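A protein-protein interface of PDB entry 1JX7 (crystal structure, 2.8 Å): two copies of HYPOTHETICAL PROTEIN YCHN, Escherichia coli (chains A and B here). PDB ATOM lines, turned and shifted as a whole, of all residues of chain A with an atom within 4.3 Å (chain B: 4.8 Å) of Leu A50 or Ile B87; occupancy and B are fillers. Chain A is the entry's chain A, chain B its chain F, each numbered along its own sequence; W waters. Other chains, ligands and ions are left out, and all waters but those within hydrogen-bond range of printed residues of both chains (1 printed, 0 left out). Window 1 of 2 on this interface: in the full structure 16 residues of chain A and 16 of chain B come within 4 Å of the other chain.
Leu A50 touches Ile B87, but with the chains exchanged Ile A87 does not touch Leu B50 (4.4 Å).
Leu A90 touches its own counterpart, Leu B90.
Of the 5 pairs that touch across the chains among the printed residues, 1 has its exchanged pair printed and touching as well.
Ile B87 touches just one residue of chain A: Leu A50.
Printed residues of chain B within 4 Å of Gln A53: Arg B85.
Printed residues of chain A within 4 Å of Arg B85: Leu A50 (3.9 Å) and Gln A53 (3.9 Å).
Of the printed residues of chain B, Leu A90 touches Leu B90 (3.4 Å).
The nearest residue of chain B that does not touch Leu A50 is Leu B90 (4.2 Å).
Hydrophobic or aromatic side chains of chain A within 4 Å of the printed part of chain B: Leu A50 and Leu A90.
Along chain B the printed residues that touch a printed residue of chain A span positions 85 to 90.
Water W1 lies within hydrogen-bond range of the backbone carbonyl oxygen (O) of Arg B85 (2.8 Å) and the backbone carbonyl oxygen (O) of Thr A47 (3.4 Å).
CB of Leu A50 touches O of Arg B85 (3.9 Å).
CD1 of Ile B87 touches CD1 of Leu A50, 3.5 Å away.
Gly B86 touches Gly A52 (CA to O, 3.8 Å).
Gln A53 touches Arg B85 (CG to O, 3.9 Å).
CD1 of Leu A90 touches CD1 of Leu B90 (3.4 Å).
N of Gln A53 lies close to NE2 of Gln A62 (2.8 Å).
The side-chain amide nitrogen (NE2) of Gln A53 lies within hydrogen-bond range of the backbone carbonyl oxygen (O) of Ala A48 (2.9 Å).
The side-chain amide nitrogen (NE2) of Gln A53 sits at hydrogen-bond distance from the backbone carbonyl oxygen (O) of Leu A50 (2.8 Å).
The backbone carbonyl oxygen (O) of Thr B82 sits at hydrogen-bond distance from the backbone NH (N) of Ile B87.
The backbone NH (N) of Gly A52 sits close to the side-chain amide nitrogen (NE2) of Gln A62, 2.6 Å away.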
ATOM      1  N   THR A  47       2.052 -11.754  -1.427  1.00  0.00           N
ATOM      2  CA  THR A  47       1.304 -12.923  -0.978  1.00  0.00           C
ATOM      3  C   THR A  47       0.447 -12.531   0.219  1.00  0.00           C
ATOM      4  O   THR A  47      -0.503 -13.241   0.566  1.00  0.00           O
ATOM      5  CB  THR A  47       2.262 -14.107  -0.602  1.00  0.00           C
ATOM      6  OG1 THR A  47       3.119 -13.730   0.481  1.00  0.00           O
ATOM      7  CG2 THR A  47       3.126 -14.496  -1.776  1.00  0.00           C
ATOM      8  N   ALA A  48       0.772 -11.385   0.820  1.00  0.00           N
ATOM      9  CA  ALA A  48       0.031 -10.850   1.965  1.00  0.00           C
ATOM     10  C   ALA A  48      -1.442 -10.574   1.627  1.00  0.00           C
ATOM     11  O   ALA A  48      -2.284 -10.378   2.513  1.00  0.00           O
ATOM     12  CB  ALA A  48       0.689  -9.575   2.432  1.00  0.00           C
ATOM     13  N   GLY A  49      -1.748 -10.555   0.331  1.00  0.00           N
ATOM     14  CA  GLY A  49      -3.107 -10.295  -0.080  1.00  0.00           C
ATOM     15  C   GLY A  49      -4.008 -11.521  -0.102  1.00  0.00           C
ATOM     16  O   GLY A  49      -5.207 -11.396  -0.368  1.00  0.00           O
ATOM     17  N   LEU A  50      -3.462 -12.700   0.175  1.00  0.00           N
ATOM     18  CA  LEU A  50      -4.301 -13.892   0.151  1.00  0.00           C
ATOM     19  C   LEU A  50      -5.291 -13.892   1.284  1.00  0.00           C
ATOM     20  O   LEU A  50      -5.039 -13.329   2.346  1.00  0.00           O
ATOM     21  CB  LEU A  50      -3.456 -15.158   0.207  1.00  0.00           C
ATOM     22  CG  LEU A  50      -2.659 -15.436  -1.065  1.00  0.00           C
ATOM     23  CD1 LEU A  50      -1.855 -16.702  -0.879  1.00  0.00           C
ATOM     24  CD2 LEU A  50      -3.591 -15.551  -2.251  1.00  0.00           C
ATOM     25  N   ARG A  51      -6.426 -14.536   1.043  1.00  0.00           N
ATOM     26  CA  ARG A  51      -7.485 -14.610   2.043  1.00  0.00           C
ATOM     27  C   ARG A  51      -7.315 -15.897   2.847  1.00  0.00           C
ATOM     28  O   ARG A  51      -6.614 -16.818   2.417  1.00  0.00           O
ATOM     29  CB  ARG A  51      -8.851 -14.599   1.340  1.00  0.00           C
ATOM     30  CG  ARG A  51     -10.005 -14.247   2.259  1.00  0.00           C
ATOM     31  CD  ARG A  51     -11.329 -14.813   1.776  1.00  0.00           C
ATOM     32  NE  ARG A  51     -12.183 -13.804   1.162  1.00  0.00           N
ATOM     33  CZ  ARG A  51     -11.843 -13.091   0.097  1.00  0.00           C
ATOM     34  NH1 ARG A  51     -10.653 -13.257  -0.470  1.00  0.00           N
ATOM     35  NH2 ARG A  51     -12.702 -12.212  -0.410  1.00  0.00           N
ATOM     36  N   GLY A  52      -7.939 -15.954   4.022  1.00  0.00           N
ATOM     37  CA  GLY A  52      -7.871 -17.150   4.844  1.00  0.00           C
ATOM     38  C   GLY A  52      -6.666 -17.294   5.760  1.00  0.00           C
ATOM     39  O   GLY A  52      -6.407 -18.376   6.280  1.00  0.00           O
ATOM     40  N   GLN A  53      -5.926 -16.203   5.954  1.00  0.00           N
ATOM     41  CA  GLN A  53      -4.760 -16.236   6.817  1.00  0.00           C
ATOM     42  C   GLN A  53      -5.242 -16.488   8.235  1.00  0.00           C
ATOM     43  O   GLN A  53      -6.112 -15.778   8.747  1.00  0.00           O
ATOM     44  CB  GLN A  53      -3.996 -14.906   6.741  1.00  0.00           C
ATOM     45  CG  GLN A  53      -3.492 -14.608   5.342  1.00  0.00           C
ATOM     46  CD  GLN A  53      -2.766 -13.284   5.232  1.00  0.00           C
ATOM     47  OE1 GLN A  53      -1.828 -13.008   5.981  1.00  0.00           O
ATOM     48  NE2 GLN A  53      -3.193 -12.464   4.274  1.00  0.00           N
ATOM     49  N   GLN A  62      -3.653 -10.326   7.640  1.00  0.00           N
ATOM     50  CA  GLN A  62      -4.927 -10.223   6.947  1.00  0.00           C
ATOM     51  C   GLN A  62      -5.786  -9.164   7.611  1.00  0.00           C
ATOM     52  O   GLN A  62      -6.330  -8.293   6.941  1.00  0.00           O
ATOM     53  CB  GLN A  62      -5.643 -11.559   6.989  1.00  0.00           C
ATOM     54  CG  GLN A  62      -6.351 -11.872   5.710  1.00  0.00           C
ATOM     55  CD  GLN A  62      -7.619 -12.640   5.923  1.00  0.00           C
ATOM     56  OE1 GLN A  62      -8.639 -12.071   6.293  1.00  0.00           O
ATOM     57  NE2 GLN A  62      -7.565 -13.948   5.704  1.00  0.00           N
ATOM     58  N   ILE A  87      -0.686 -15.776  -7.764  1.00  0.00           N
ATOM     59  CA  ILE A  87      -1.626 -15.201  -6.821  1.00  0.00           C
ATOM     60  C   ILE A  87      -2.633 -14.322  -7.546  1.00  0.00           C
ATOM     61  O   ILE A  87      -3.669 -13.972  -6.982  1.00  0.00           O
ATOM     62  CB  ILE A  87      -0.838 -14.419  -5.771  1.00  0.00           C
ATOM     63  CG1 ILE A  87      -0.180 -15.423  -4.829  1.00  0.00           C
ATOM     64  CG2 ILE A  87      -1.719 -13.432  -5.045  1.00  0.00           C
ATOM     65  CD1 ILE A  87       0.704 -14.803  -3.792  1.00  0.00           C
ATOM     66  N   LEU A  90      -6.081 -15.892  -7.518  1.00  0.00           N
ATOM     67  CA  LEU A  90      -6.571 -16.359  -6.242  1.00  0.00           C
ATOM     68  C   LEU A  90      -7.475 -15.317  -5.601  1.00  0.00           C
ATOM     69  O   LEU A  90      -7.517 -14.164  -6.032  1.00  0.00           O
ATOM     70  CB  LEU A  90      -5.407 -16.683  -5.300  1.00  0.00           C
ATOM     71  CG  LEU A  90      -4.513 -17.825  -5.779  1.00  0.00           C
ATOM     72  CD1 LEU A  90      -3.616 -18.265  -4.638  1.00  0.00           C
ATOM     73  CD2 LEU A  90      -5.362 -18.996  -6.245  1.00  0.00           C
ATOM     74  N   PRO A  91      -8.249 -15.729  -4.569  1.00  0.00           N
ATOM     75  CA  PRO A  91      -9.156 -14.815  -3.869  1.00  0.00           C
ATOM     76  C   PRO A  91      -8.345 -13.885  -2.973  1.00  0.00           C
ATOM     77  O   PRO A  91      -7.628 -14.341  -2.079  1.00  0.00           O
ATOM     78  CB  PRO A  91     -10.040 -15.767  -3.060  1.00  0.00           C
ATOM     79  CG  PRO A  91      -9.986 -17.059  -3.851  1.00  0.00           C
ATOM     80  CD  PRO A  91      -8.529 -17.128  -4.201  1.00  0.00           C
ATOM     81  N   ILE A  93      -8.019 -10.555  -0.280  1.00  0.00           N
ATOM     82  CA  ILE A  93      -8.756  -9.930   0.821  1.00  0.00           C
ATOM     83  C   ILE A  93      -9.525  -8.801   0.145  1.00  0.00           C
ATOM     84  O   ILE A  93      -9.072  -8.256  -0.859  1.00  0.00           O
ATOM     85  CB  ILE A  93      -7.777  -9.355   1.863  1.00  0.00           C
ATOM     86  CG1 ILE A  93      -6.838 -10.464   2.351  1.00  0.00           C
ATOM     87  CG2 ILE A  93      -8.542  -8.745   3.017  1.00  0.00           C
ATOM     88  CD1 ILE A  93      -5.782  -9.997   3.338  1.00  0.00           C
ATOM     89  N   VAL B  46       7.155 -21.501   1.927  1.00  0.00           N
ATOM     90  CA  VAL B  46       5.899 -22.235   1.812  1.00  0.00           C
ATOM     91  C   VAL B  46       5.005 -21.855   0.620  1.00  0.00           C
ATOM     92  O   VAL B  46       4.306 -22.699   0.066  1.00  0.00           O
ATOM     93  CB  VAL B  46       5.108 -22.102   3.133  1.00  0.00           C
ATOM     94  CG1 VAL B  46       3.648 -22.322   2.901  1.00  0.00           C
ATOM     95  CG2 VAL B  46       5.626 -23.113   4.136  1.00  0.00           C
ATOM     96  N   THR B  47       5.029 -20.597   0.238  1.00  0.00           N
ATOM     97  CA  THR B  47       4.204 -20.139  -0.886  1.00  0.00           C
ATOM     98  C   THR B  47       4.713 -20.641  -2.250  1.00  0.00           C
ATOM     99  O   THR B  47       4.031 -20.504  -3.268  1.00  0.00           O
ATOM    100  CB  THR B  47       4.118 -18.596  -0.895  1.00  0.00           C
ATOM    101  OG1 THR B  47       5.443 -18.047  -0.874  1.00  0.00           O
ATOM    102  CG2 THR B  47       3.352 -18.093   0.325  1.00  0.00           C
ATOM    103  N   LEU B  50       2.565 -23.197  -4.405  1.00  0.00           N
ATOM    104  CA  LEU B  50       1.311 -22.850  -5.068  1.00  0.00           C
ATOM    105  C   LEU B  50       1.342 -23.098  -6.563  1.00  0.00           C
ATOM    106  O   LEU B  50       2.392 -23.041  -7.200  1.00  0.00           O
ATOM    107  CB  LEU B  50       0.956 -21.383  -4.813  1.00  0.00           C
ATOM    108  CG  LEU B  50       0.295 -21.060  -3.484  1.00  0.00           C
ATOM    109  CD1 LEU B  50       0.024 -19.566  -3.424  1.00  0.00           C
ATOM    110  CD2 LEU B  50      -0.998 -21.841  -3.348  1.00  0.00           C
ATOM    111  N   LEU B  77       5.514 -28.972   2.909  1.00  0.00           N
ATOM    112  CA  LEU B  77       5.303 -27.605   3.368  1.00  0.00           C
ATOM    113  C   LEU B  77       4.900 -27.637   4.841  1.00  0.00           C
ATOM    114  O   LEU B  77       3.983 -28.362   5.222  1.00  0.00           O
ATOM    115  CB  LEU B  77       4.186 -26.921   2.561  1.00  0.00           C
ATOM    116  CG  LEU B  77       4.268 -26.915   1.041  1.00  0.00           C
ATOM    117  CD1 LEU B  77       3.139 -26.051   0.507  1.00  0.00           C
ATOM    118  CD2 LEU B  77       5.622 -26.382   0.569  1.00  0.00           C
ATOM    119  N   THR B  82       1.940 -22.652   6.555  1.00  0.00           N
ATOM    120  CA  THR B  82       0.914 -22.650   5.514  1.00  0.00           C
ATOM    121  C   THR B  82      -0.402 -22.093   6.043  1.00  0.00           C
ATOM    122  O   THR B  82      -1.071 -21.335   5.342  1.00  0.00           O
ATOM    123  CB  THR B  82       0.650 -24.062   4.954  1.00  0.00           C
ATOM    124  OG1 THR B  82       0.290 -24.956   6.023  1.00  0.00           O
ATOM    125  CG2 THR B  82       1.875 -24.583   4.216  1.00  0.00           C
ATOM    126  N   ARG B  85      -0.603 -18.293   6.293  1.00  0.00           N
ATOM    127  CA  ARG B  85      -0.533 -17.592   5.022  1.00  0.00           C
ATOM    128  C   ARG B  85      -1.700 -17.960   4.130  1.00  0.00           C
ATOM    129  O   ARG B  85      -1.877 -17.376   3.062  1.00  0.00           O
ATOM    130  CB  ARG B  85       0.779 -17.903   4.320  1.00  0.00           C
ATOM    131  CG  ARG B  85       1.980 -17.450   5.091  1.00  0.00           C
ATOM    132  CD  ARG B  85       3.205 -18.265   4.750  1.00  0.00           C
ATOM    133  NE  ARG B  85       4.067 -18.371   5.920  1.00  0.00           N
ATOM    134  CZ  ARG B  85       5.088 -17.566   6.165  1.00  0.00           C
ATOM    135  NH1 ARG B  85       5.389 -16.595   5.301  1.00  0.00           N
ATOM    136  NH2 ARG B  85       5.793 -17.718   7.274  1.00  0.00           N
ATOM    137  N   GLY B  86      -2.502 -18.920   4.578  1.00  0.00           N
ATOM    138  CA  GLY B  86      -3.648 -19.343   3.807  1.00  0.00           C
ATOM    139  C   GLY B  86      -3.273 -20.161   2.591  1.00  0.00           C
ATOM    140  O   GLY B  86      -3.947 -20.098   1.573  1.00  0.00           O
ATOM    141  N   ILE B  87      -2.192 -20.927   2.696  1.00  0.00           N
ATOM    142  CA  ILE B  87      -1.714 -21.775   1.604  1.00  0.00           C
ATOM    143  C   ILE B  87      -2.189 -23.227   1.781  1.00  0.00           C
ATOM    144  O   ILE B  87      -2.225 -23.992   0.811  1.00  0.00           O
ATOM    145  CB  ILE B  87      -0.142 -21.748   1.518  1.00  0.00           C
ATOM    146  CG1 ILE B  87       0.315 -20.626   0.586  1.00  0.00           C
ATOM    147  CG2 ILE B  87       0.403 -23.072   1.002  1.00  0.00           C
ATOM    148  CD1 ILE B  87      -0.225 -19.259   0.943  1.00  0.00           C
ATOM    149  N   SER B  88      -2.555 -23.589   3.006  1.00  0.00           N
ATOM    150  CA  SER B  88      -2.998 -24.938   3.352  1.00  0.00           C
ATOM    151  C   SER B  88      -4.172 -25.444   2.516  1.00  0.00           C
ATOM    152  O   SER B  88      -4.126 -26.537   1.943  1.00  0.00           O
ATOM    153  CB  SER B  88      -3.405 -25.003   4.829  1.00  0.00           C
ATOM    154  OG  SER B  88      -2.395 -24.485   5.672  1.00  0.00           O
ATOM    155  N   THR B  89      -5.227 -24.642   2.475  1.00  0.00           N
ATOM    156  CA  THR B  89      -6.439 -24.986   1.757  1.00  0.00           C
ATOM    157  C   THR B  89      -6.366 -24.787   0.248  1.00  0.00           C
ATOM    158  O   THR B  89      -7.113 -25.420  -0.498  1.00  0.00           O
ATOM    159  CB  THR B  89      -7.617 -24.175   2.311  1.00  0.00           C
ATOM    160  OG1 THR B  89      -7.237 -22.793   2.420  1.00  0.00           O
ATOM    161  CG2 THR B  89      -8.011 -24.698   3.680  1.00  0.00           C
ATOM    162  N   LEU B  90      -5.468 -23.912  -0.198  1.00  0.00           N
ATOM    163  CA  LEU B  90      -5.304 -23.636  -1.622  1.00  0.00           C
ATOM    164  C   LEU B  90      -4.648 -24.780  -2.413  1.00  0.00           C
ATOM    165  O   LEU B  90      -4.033 -25.683  -1.837  1.00  0.00           O
ATOM    166  CB  LEU B  90      -4.503 -22.339  -1.812  1.00  0.00           C
ATOM    167  CG  LEU B  90      -5.214 -21.059  -1.339  1.00  0.00           C
ATOM    168  CD1 LEU B  90      -4.441 -19.841  -1.794  1.00  0.00           C
ATOM    169  CD2 LEU B  90      -6.625 -21.014  -1.898  1.00  0.00           C
ATOM    170  N   LEU B  92      -2.117 -26.940  -4.376  1.00  0.00           N
ATOM    171  CA  LEU B  92      -0.671 -27.102  -4.368  1.00  0.00           C
ATOM    172  C   LEU B  92      -0.074 -27.704  -5.644  1.00  0.00           C
ATOM    173  O   LEU B  92      -0.745 -28.428  -6.378  1.00  0.00           O
ATOM    174  CB  LEU B  92      -0.276 -27.937  -3.148  1.00  0.00           C
ATOM    175  CG  LEU B  92      -0.022 -27.175  -1.836  1.00  0.00           C
ATOM    176  CD1 LEU B  92      -0.861 -25.900  -1.755  1.00  0.00           C
ATOM    177  CD2 LEU B  92      -0.313 -28.111  -0.664  1.00  0.00           C
HETATM  178  O   HOH W   1      -0.198 -15.165   3.390  1.00  0.00           O
